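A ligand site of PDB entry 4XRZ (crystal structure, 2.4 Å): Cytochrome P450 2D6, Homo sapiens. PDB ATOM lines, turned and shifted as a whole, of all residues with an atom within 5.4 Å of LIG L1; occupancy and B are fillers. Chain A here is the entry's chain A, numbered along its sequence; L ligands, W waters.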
ATOM      1  N   PHE A  98     -22.333  -7.796 -10.468  1.00  0.00           N
ATOM      2  CA  PHE A  98     -22.277  -9.243 -10.288  1.00  0.00           C
ATOM      3  C   PHE A  98     -20.870  -9.831 -10.376  1.00  0.00           C
ATOM      4  O   PHE A  98     -20.429 -10.514  -9.453  1.00  0.00           O
ATOM      5  CB  PHE A  98     -23.170  -9.925 -11.316  1.00  0.00           C
ATOM      6  CG  PHE A  98     -24.217 -10.809 -10.699  1.00  0.00           C
ATOM      7  CD1 PHE A  98     -25.501 -10.338 -10.518  1.00  0.00           C
ATOM      8  CD2 PHE A  98     -23.906 -12.098 -10.305  1.00  0.00           C
ATOM      9  CE1 PHE A  98     -26.466 -11.150  -9.953  1.00  0.00           C
ATOM     10  CE2 PHE A  98     -24.864 -12.908  -9.734  1.00  0.00           C
ATOM     11  CZ  PHE A  98     -26.147 -12.428  -9.556  1.00  0.00           C
ATOM     12  N   LEU A  99     -20.185  -9.566 -11.484  1.00  0.00           N
ATOM     13  CA  LEU A  99     -18.855 -10.121 -11.691  1.00  0.00           C
ATOM     14  C   LEU A  99     -17.762  -9.094 -11.422  1.00  0.00           C
ATOM     15  O   LEU A  99     -16.582  -9.347 -11.675  1.00  0.00           O
ATOM     16  CB  LEU A  99     -18.717 -10.660 -13.120  1.00  0.00           C
ATOM     17  CG  LEU A  99     -19.666 -11.791 -13.487  1.00  0.00           C
ATOM     18  CD1 LEU A  99     -19.378 -12.276 -14.905  1.00  0.00           C
ATOM     19  CD2 LEU A  99     -19.561 -12.947 -12.487  1.00  0.00           C
ATOM     20  N   LEU A 186     -34.548 -14.834 -24.865  1.00  0.00           N
ATOM     21  CA  LEU A 186     -33.087 -14.724 -24.944  1.00  0.00           C
ATOM     22  C   LEU A 186     -32.446 -14.806 -23.565  1.00  0.00           C
ATOM     23  O   LEU A 186     -31.399 -15.437 -23.399  1.00  0.00           O
ATOM     24  CB  LEU A 186     -32.699 -13.408 -25.625  1.00  0.00           C
ATOM     25  CG  LEU A 186     -33.040 -13.298 -27.113  1.00  0.00           C
ATOM     26  CD1 LEU A 186     -32.662 -11.928 -27.645  1.00  0.00           C
ATOM     27  CD2 LEU A 186     -32.345 -14.404 -27.903  1.00  0.00           C
ATOM     28  N   ALA A 187     -33.074 -14.163 -22.590  1.00  0.00           N
ATOM     29  CA  ALA A 187     -32.583 -14.172 -21.216  1.00  0.00           C
ATOM     30  C   ALA A 187     -32.549 -15.589 -20.657  1.00  0.00           C
ATOM     31  O   ALA A 187     -31.629 -15.960 -19.930  1.00  0.00           O
ATOM     32  CB  ALA A 187     -33.435 -13.277 -20.332  1.00  0.00           C
ATOM     33  N   GLU A 189     -32.386 -18.423 -22.482  1.00  0.00           N
ATOM     34  CA  GLU A 189     -31.368 -19.151 -23.217  1.00  0.00           C
ATOM     35  C   GLU A 189     -29.966 -18.717 -22.783  1.00  0.00           C
ATOM     36  O   GLU A 189     -29.029 -19.506 -22.789  1.00  0.00           O
ATOM     37  CB  GLU A 189     -31.530 -18.956 -24.720  1.00  0.00           C
ATOM     38  CG  GLU A 189     -32.774 -19.612 -25.294  1.00  0.00           C
ATOM     39  CD  GLU A 189     -32.745 -21.119 -25.182  1.00  0.00           C
ATOM     40  OE1 GLU A 189     -31.648 -21.704 -25.235  1.00  0.00           O
ATOM     41  OE2 GLU A 189     -33.830 -21.728 -25.025  1.00  0.00           O
ATOM     42  N   GLY A 190     -29.851 -17.451 -22.398  1.00  0.00           N
ATOM     43  CA  GLY A 190     -28.585 -16.926 -21.908  1.00  0.00           C
ATOM     44  C   GLY A 190     -28.227 -17.518 -20.558  1.00  0.00           C
ATOM     45  O   GLY A 190     -27.059 -17.619 -20.195  1.00  0.00           O
ATOM     46  N   LEU A 191     -29.255 -17.912 -19.802  1.00  0.00           N
ATOM     47  CA  LEU A 191     -29.061 -18.526 -18.501  1.00  0.00           C
ATOM     48  C   LEU A 191     -28.432 -19.903 -18.636  1.00  0.00           C
ATOM     49  O   LEU A 191     -27.634 -20.314 -17.795  1.00  0.00           O
ATOM     50  CB  LEU A 191     -30.393 -18.627 -17.758  1.00  0.00           C
ATOM     51  CG  LEU A 191     -30.330 -19.218 -16.345  1.00  0.00           C
ATOM     52  CD1 LEU A 191     -29.408 -18.403 -15.463  1.00  0.00           C
ATOM     53  CD2 LEU A 191     -31.724 -19.313 -15.737  1.00  0.00           C
ATOM     54  N   GLU A 194     -24.811 -19.835 -19.015  1.00  0.00           N
ATOM     55  CA  GLU A 194     -24.122 -19.572 -17.763  1.00  0.00           C
ATOM     56  C   GLU A 194     -23.623 -20.874 -17.150  1.00  0.00           C
ATOM     57  O   GLU A 194     -22.811 -20.875 -16.228  1.00  0.00           O
ATOM     58  CB  GLU A 194     -25.040 -18.832 -16.783  1.00  0.00           C
ATOM     59  CG  GLU A 194     -24.311 -18.071 -15.678  1.00  0.00           C
ATOM     60  CD  GLU A 194     -23.721 -16.755 -16.160  1.00  0.00           C
ATOM     61  OE1 GLU A 194     -23.772 -16.475 -17.382  1.00  0.00           O
ATOM     62  OE2 GLU A 194     -23.200 -16.001 -15.311  1.00  0.00           O
ATOM     63  N   GLN A 222     -26.570 -14.623 -25.026  1.00  0.00           N
ATOM     64  CA  GLN A 222     -26.313 -13.523 -24.105  1.00  0.00           C
ATOM     65  C   GLN A 222     -25.978 -12.240 -24.874  1.00  0.00           C
ATOM     66  O   GLN A 222     -26.350 -11.146 -24.458  1.00  0.00           O
ATOM     67  CB  GLN A 222     -25.176 -13.862 -23.138  1.00  0.00           C
ATOM     68  CG  GLN A 222     -25.540 -14.902 -22.087  1.00  0.00           C
ATOM     69  CD  GLN A 222     -24.466 -15.076 -21.042  1.00  0.00           C
ATOM     70  OE1 GLN A 222     -23.519 -14.282 -20.963  1.00  0.00           O
ATOM     71  NE2 GLN A 222     -24.578 -16.113 -20.228  1.00  0.00           N
ATOM     72  N   ALA A 278     -28.839  -4.981 -17.597  1.00  0.00           N
ATOM     73  CA  ALA A 278     -28.970  -6.371 -18.019  1.00  0.00           C
ATOM     74  C   ALA A 278     -28.950  -7.320 -16.839  1.00  0.00           C
ATOM     75  O   ALA A 278     -29.773  -8.230 -16.743  1.00  0.00           O
ATOM     76  CB  ALA A 278     -27.864  -6.740 -19.001  1.00  0.00           C
ATOM     77  N   ASP A 279     -28.009  -7.095 -15.930  1.00  0.00           N
ATOM     78  CA  ASP A 279     -27.898  -7.934 -14.740  1.00  0.00           C
ATOM     79  C   ASP A 279     -29.133  -7.818 -13.870  1.00  0.00           C
ATOM     80  O   ASP A 279     -29.672  -8.832 -13.414  1.00  0.00           O
ATOM     81  CB  ASP A 279     -26.644  -7.574 -13.927  1.00  0.00           C
ATOM     82  CG  ASP A 279     -25.366  -8.069 -14.581  1.00  0.00           C
ATOM     83  OD1 ASP A 279     -25.445  -8.730 -15.633  1.00  0.00           O
ATOM     84  OD2 ASP A 279     -24.278  -7.794 -14.029  1.00  0.00           O
ATOM     85  N   SER A 282     -32.496  -9.327 -15.852  1.00  0.00           N
ATOM     86  CA  SER A 282     -32.445 -10.779 -15.974  1.00  0.00           C
ATOM     87  C   SER A 282     -32.493 -11.446 -14.601  1.00  0.00           C
ATOM     88  O   SER A 282     -33.098 -12.511 -14.441  1.00  0.00           O
ATOM     89  CB  SER A 282     -31.192 -11.211 -16.740  1.00  0.00           C
ATOM     90  OG  SER A 282     -30.021 -10.775 -16.080  1.00  0.00           O
ATOM     91  N   ALA A 283     -31.860 -10.826 -13.607  1.00  0.00           N
ATOM     92  CA  ALA A 283     -31.919 -11.325 -12.236  1.00  0.00           C
ATOM     93  C   ALA A 283     -33.330 -11.189 -11.700  1.00  0.00           C
ATOM     94  O   ALA A 283     -33.868 -12.114 -11.085  1.00  0.00           O
ATOM     95  CB  ALA A 283     -30.946 -10.583 -11.339  1.00  0.00           C
ATOM     96  N   VAL A 286     -35.424 -14.274 -13.678  1.00  0.00           N
ATOM     97  CA  VAL A 286     -35.231 -15.719 -13.559  1.00  0.00           C
ATOM     98  C   VAL A 286     -35.161 -16.254 -12.133  1.00  0.00           C
ATOM     99  O   VAL A 286     -35.298 -17.456 -11.920  1.00  0.00           O
ATOM    100  CB  VAL A 286     -33.947 -16.156 -14.297  1.00  0.00           C
ATOM    101  CG1 VAL A 286     -33.999 -15.702 -15.746  1.00  0.00           C
ATOM    102  CG2 VAL A 286     -32.716 -15.586 -13.594  1.00  0.00           C
ATOM    103  N   THR A 287     -34.952 -15.375 -11.158  1.00  0.00           N
ATOM    104  CA  THR A 287     -34.853 -15.809  -9.772  1.00  0.00           C
ATOM    105  C   THR A 287     -36.230 -15.923  -9.116  1.00  0.00           C
ATOM    106  O   THR A 287     -36.611 -17.000  -8.653  1.00  0.00           O
ATOM    107  CB  THR A 287     -33.996 -14.835  -8.935  1.00  0.00           C
ATOM    108  OG1 THR A 287     -34.562 -13.521  -8.996  1.00  0.00           O
ATOM    109  CG2 THR A 287     -32.560 -14.811  -9.453  1.00  0.00           C
ATOM    110  N   VAL A 348     -30.295 -21.485  -6.226  1.00  0.00           N
ATOM    111  CA  VAL A 348     -28.887 -21.184  -6.487  1.00  0.00           C
ATOM    112  C   VAL A 348     -28.012 -22.065  -5.586  1.00  0.00           C
ATOM    113  O   VAL A 348     -27.452 -21.588  -4.602  1.00  0.00           O
ATOM    114  CB  VAL A 348     -28.532 -19.705  -6.234  1.00  0.00           C
ATOM    115  CG1 VAL A 348     -27.311 -19.314  -7.055  1.00  0.00           C
ATOM    116  CG2 VAL A 348     -29.696 -18.803  -6.612  1.00  0.00           C
ATOM    117  N   VAL A 352     -22.750 -17.953  -6.099  1.00  0.00           N
ATOM    118  CA  VAL A 352     -21.862 -17.342  -7.078  1.00  0.00           C
ATOM    119  C   VAL A 352     -20.435 -17.418  -6.560  1.00  0.00           C
ATOM    120  O   VAL A 352     -20.189 -17.172  -5.378  1.00  0.00           O
ATOM    121  CB  VAL A 352     -22.266 -15.875  -7.357  1.00  0.00           C
ATOM    122  CG1 VAL A 352     -21.278 -15.222  -8.308  1.00  0.00           C
ATOM    123  CG2 VAL A 352     -23.675 -15.811  -7.911  1.00  0.00           C
ATOM    124  N   CYS A 421     -26.983 -11.089  -1.942  1.00  0.00           N
ATOM    125  CA  CYS A 421     -27.927 -10.587  -2.941  1.00  0.00           C
ATOM    126  C   CYS A 421     -28.538  -9.234  -2.564  1.00  0.00           C
ATOM    127  O   CYS A 421     -29.163  -9.092  -1.512  1.00  0.00           O
ATOM    128  CB  CYS A 421     -29.030 -11.611  -3.165  1.00  0.00           C
ATOM    129  SG  CYS A 421     -30.253 -11.128  -4.408  1.00  0.00           S
ATOM    130  N   PHE A 461     -27.072 -23.676 -13.667  1.00  0.00           N
ATOM    131  CA  PHE A 461     -26.697 -22.637 -12.705  1.00  0.00           C
ATOM    132  C   PHE A 461     -27.846 -22.391 -11.728  1.00  0.00           C
ATOM    133  O   PHE A 461     -27.683 -22.550 -10.524  1.00  0.00           O
ATOM    134  CB  PHE A 461     -26.297 -21.337 -13.398  1.00  0.00           C
ATOM    135  CG  PHE A 461     -26.035 -20.206 -12.442  1.00  0.00           C
ATOM    136  CD1 PHE A 461     -24.899 -20.210 -11.652  1.00  0.00           C
ATOM    137  CD2 PHE A 461     -26.935 -19.157 -12.323  1.00  0.00           C
ATOM    138  CE1 PHE A 461     -24.659 -19.181 -10.761  1.00  0.00           C
ATOM    139  CE2 PHE A 461     -26.695 -18.128 -11.432  1.00  0.00           C
ATOM    140  CZ  PHE A 461     -25.553 -18.135 -10.649  1.00  0.00           C
ATOM    141  N   LEU A 462     -28.989 -21.987 -12.261  1.00  0.00           N
ATOM    142  CA  LEU A 462     -30.220 -21.953 -11.495  1.00  0.00           C
ATOM    143  C   LEU A 462     -30.896 -23.310 -11.561  1.00  0.00           C
ATOM    144  O   LEU A 462     -30.804 -23.996 -12.581  1.00  0.00           O
ATOM    145  CB  LEU A 462     -31.161 -20.865 -11.996  1.00  0.00           C
ATOM    146  CG  LEU A 462     -31.459 -19.719 -11.033  1.00  0.00           C
ATOM    147  CD1 LEU A 462     -30.174 -19.081 -10.541  1.00  0.00           C
ATOM    148  CD2 LEU A 462     -32.342 -18.688 -11.710  1.00  0.00           C
HETATM  149  C1  LIG L   1     -27.032 -14.638 -17.894  1.00  0.00           C
HETATM  150  C2  LIG L   1     -26.904 -14.584 -16.510  1.00  0.00           C
HETATM  151  C3  LIG L   1     -28.010 -14.443 -15.663  1.00  0.00           C
HETATM  152  C4  LIG L   1     -29.283 -14.380 -16.291  1.00  0.00           C
HETATM  153  C5  LIG L   1     -29.447 -14.433 -17.678  1.00  0.00           C
HETATM  154  C6  LIG L   1     -28.305 -14.558 -18.461  1.00  0.00           C
HETATM  155  F1  LIG L   1     -28.424 -14.573 -19.782  1.00  0.00           F
HETATM  156  F2  LIG L   1     -30.419 -14.271 -15.594  1.00  0.00           F
HETATM  157  C7  LIG L   1     -27.807 -14.318 -14.161  1.00  0.00           C
HETATM  158  C8  LIG L   1     -28.528 -15.453 -13.420  1.00  0.00           C
HETATM  159  O1  LIG L   1     -28.511 -15.264 -12.003  1.00  0.00           O
HETATM  160  C9  LIG L   1     -29.148 -14.038 -11.602  1.00  0.00           C
HETATM  161  C10 LIG L   1     -28.377 -12.852 -12.156  1.00  0.00           C
HETATM  162  C11 LIG L   1     -28.358 -12.950 -13.684  1.00  0.00           C
HETATM  163  C12 LIG L   1     -27.583 -11.789 -14.320  1.00  0.00           C
HETATM  164  S1  LIG L   1     -25.807 -11.789 -13.981  1.00  0.00           S
HETATM  165  C13 LIG L   1     -25.523 -13.544 -13.754  1.00  0.00           C
HETATM  166  N1  LIG L   1     -26.374 -14.525 -13.835  1.00  0.00           N
HETATM  167  N2  LIG L   1     -24.215 -13.816 -13.470  1.00  0.00           N
HETATM  168  C14 LIG L   1     -29.110 -14.048 -10.108  1.00  0.00           C
HETATM  169  C15 LIG L   1     -28.724 -15.102  -9.287  1.00  0.00           C
HETATM  170  N3  LIG L   1     -28.859 -14.634  -7.993  1.00  0.00           N
HETATM  171  N4  LIG L   1     -29.312 -13.356  -7.931  1.00  0.00           N
HETATM  172  C16 LIG L   1     -29.473 -12.974  -9.229  1.00  0.00           C
HETATM  173  C1  LG2 L   2     -26.271 -12.001  -5.853  1.00  0.00           C
HETATM  174  C2  LG2 L   2     -29.715 -15.244  -4.738  1.00  0.00           C
HETATM  175  C3  LG2 L   2     -33.083 -12.230  -6.494  1.00  0.00           C
HETATM  176  C4  LG2 L   2     -29.613  -9.192  -7.975  1.00  0.00           C
HETATM  177  C5  LG2 L   2     -26.891 -13.160  -5.413  1.00  0.00           C
HETATM  178  C6  LG2 L   2     -26.244 -14.345  -4.895  1.00  0.00           C
HETATM  179  C7  LG2 L   2     -27.197 -15.235  -4.590  1.00  0.00           C
HETATM  180  C8  LG2 L   2     -28.481 -14.649  -4.901  1.00  0.00           C
HETATM  181  C9  LG2 L   2     -26.951 -16.612  -4.016  1.00  0.00           C
HETATM  182  C10 LG2 L   2     -24.725 -14.544  -4.729  1.00  0.00           C
HETATM  183  C11 LG2 L   2     -24.174 -13.783  -3.530  1.00  0.00           C
HETATM  184  C12 LG2 L   2     -22.693 -14.052  -3.399  1.00  0.00           C
HETATM  185  O1  LG2 L   2     -21.936 -13.662  -4.315  1.00  0.00           O
HETATM  186  O2  LG2 L   2     -22.266 -14.666  -2.391  1.00  0.00           O
HETATM  187  C13 LG2 L   2     -30.946 -14.720  -5.104  1.00  0.00           C
HETATM  188  C14 LG2 L   2     -32.244 -15.335  -4.920  1.00  0.00           C
HETATM  189  C15 LG2 L   2     -33.175 -14.498  -5.418  1.00  0.00           C
HETATM  190  C16 LG2 L   2     -32.487 -13.329  -5.913  1.00  0.00           C
HETATM  191  C17 LG2 L   2     -32.434 -16.701  -4.285  1.00  0.00           C
HETATM  192  C18 LG2 L   2     -34.721 -14.634  -5.484  1.00  0.00           C
HETATM  193  C19 LG2 L   2     -35.436 -15.646  -5.001  1.00  0.00           C
HETATM  194  C20 LG2 L   2     -32.456 -11.131  -7.028  1.00  0.00           C
HETATM  195  C21 LG2 L   2     -33.094  -9.963  -7.602  1.00  0.00           C
HETATM  196  C22 LG2 L   2     -32.134  -9.118  -8.020  1.00  0.00           C
HETATM  197  C23 LG2 L   2     -30.854  -9.737  -7.714  1.00  0.00           C
HETATM  198  C24 LG2 L   2     -34.596  -9.794  -7.687  1.00  0.00           C
HETATM  199  C25 LG2 L   2     -32.252  -7.728  -8.694  1.00  0.00           C
HETATM  200  C26 LG2 L   2     -33.390  -7.087  -8.956  1.00  0.00           C
HETATM  201  C27 LG2 L   2     -28.411  -9.671  -7.500  1.00  0.00           C
HETATM  202  C28 LG2 L   2     -27.125  -9.007  -7.630  1.00  0.00           C
HETATM  203  C29 LG2 L   2     -26.209  -9.786  -7.044  1.00  0.00           C
HETATM  204  C30 LG2 L   2     -26.874 -10.960  -6.528  1.00  0.00           C
HETATM  205  C31 LG2 L   2     -26.865  -7.692  -8.310  1.00  0.00           C
HETATM  206  C32 LG2 L   2     -24.692  -9.489  -6.939  1.00  0.00           C
HETATM  207  C33 LG2 L   2     -24.417  -8.713  -5.654  1.00  0.00           C
HETATM  208  C34 LG2 L   2     -22.933  -8.461  -5.532  1.00  0.00           C
HETATM  209  O3  LG2 L   2     -22.524  -7.601  -4.708  1.00  0.00           O
HETATM  210  O4  LG2 L   2     -22.156  -9.108  -6.271  1.00  0.00           O
HETATM  211  N1  LG2 L   2     -28.254 -13.382  -5.402  1.00  0.00           N
HETATM  212  N2  LG2 L   2     -31.131 -13.493  -5.709  1.00  0.00           N
HETATM  213  N3  LG2 L   2     -31.089 -10.953  -7.116  1.00  0.00           N
HETATM  214  N4  LG2 L   2     -28.214 -10.855  -6.820  1.00  0.00           N
HETATM  215 FE1  LG2 L   2     -29.670 -12.224  -6.291  1.00  0.00          FE
HETATM  216  O   HOH W   1     -23.073 -10.178 -15.391  1.00  0.00           O
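The side-chain carboxylate (OE2) of Glu 194 lies within hydrogen-bond range of a nitrogen (N2) of LIG L1 (3.0 Å). FE1 of LG2 L2 is bound by SG of Cys 421 (2.3 Å).
N4 of LIG L1 binds FE1 of LG2 L2 (2.0 Å).
The side-chain carboxylate (OE1) of Glu 194 is in hydrogen-bond range of the side-chain amide nitrogen (NE2) of Gln 222 (3.0 Å). The side-chain amide nitrogen (NE2) of Gln 222 is in hydrogen-bond range of the backbone carbonyl oxygen (O) of Gly 190 (2.9 Å). The backbone carbonyl oxygen (O) of Asp 279 is in hydrogen-bond range of the side-chain hydroxyl (OG) of Ser 282. The backbone carbonyl oxygen (O) of Ala 278 lies within hydrogen-bond range of the side-chain hydroxyl (OG) of Ser 282, at 2.6 Å. The side-chain hydroxyl of Thr 287 lies within hydrogen-bond range of the backbone carbonyl oxygen of Ala 283, 2.6 Å away.
A fluorine (F1) of LIG L1 sits close to the backbone carbonyl oxygen of Ala 187 (3.5 Å). The backbone carbonyl oxygen (O) of Gly 190 lies close to a fluorine (F1) of LIG L1, 3.4 Å away. The backbone NH (N) of Leu 191 sits close to a fluorine (F1) of LIG L1 (3.4 Å). The side-chain carboxylate of Asp 279 lies close to a sulfur (S1) of LIG L1 (3.5 Å). O of Ser 282 sits close to F2 of LIG L1 (3.4 Å). Residues that only touch LIG L1: Phe 98, Gln 222, Ala 283, Val 286, Thr 287 and Phe 461. Hydrophobic or aromatic side chains that line LIG L1: Phe 98, Leu 191, Ala 283, Val 286 and Phe 461. The nearest printed residue that does not touch LIG L1 is Cys 421 (4.3 Å).
Water W1 lies within hydrogen-bond range of OD1 of Asp 279 and S1 of LIG L1.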
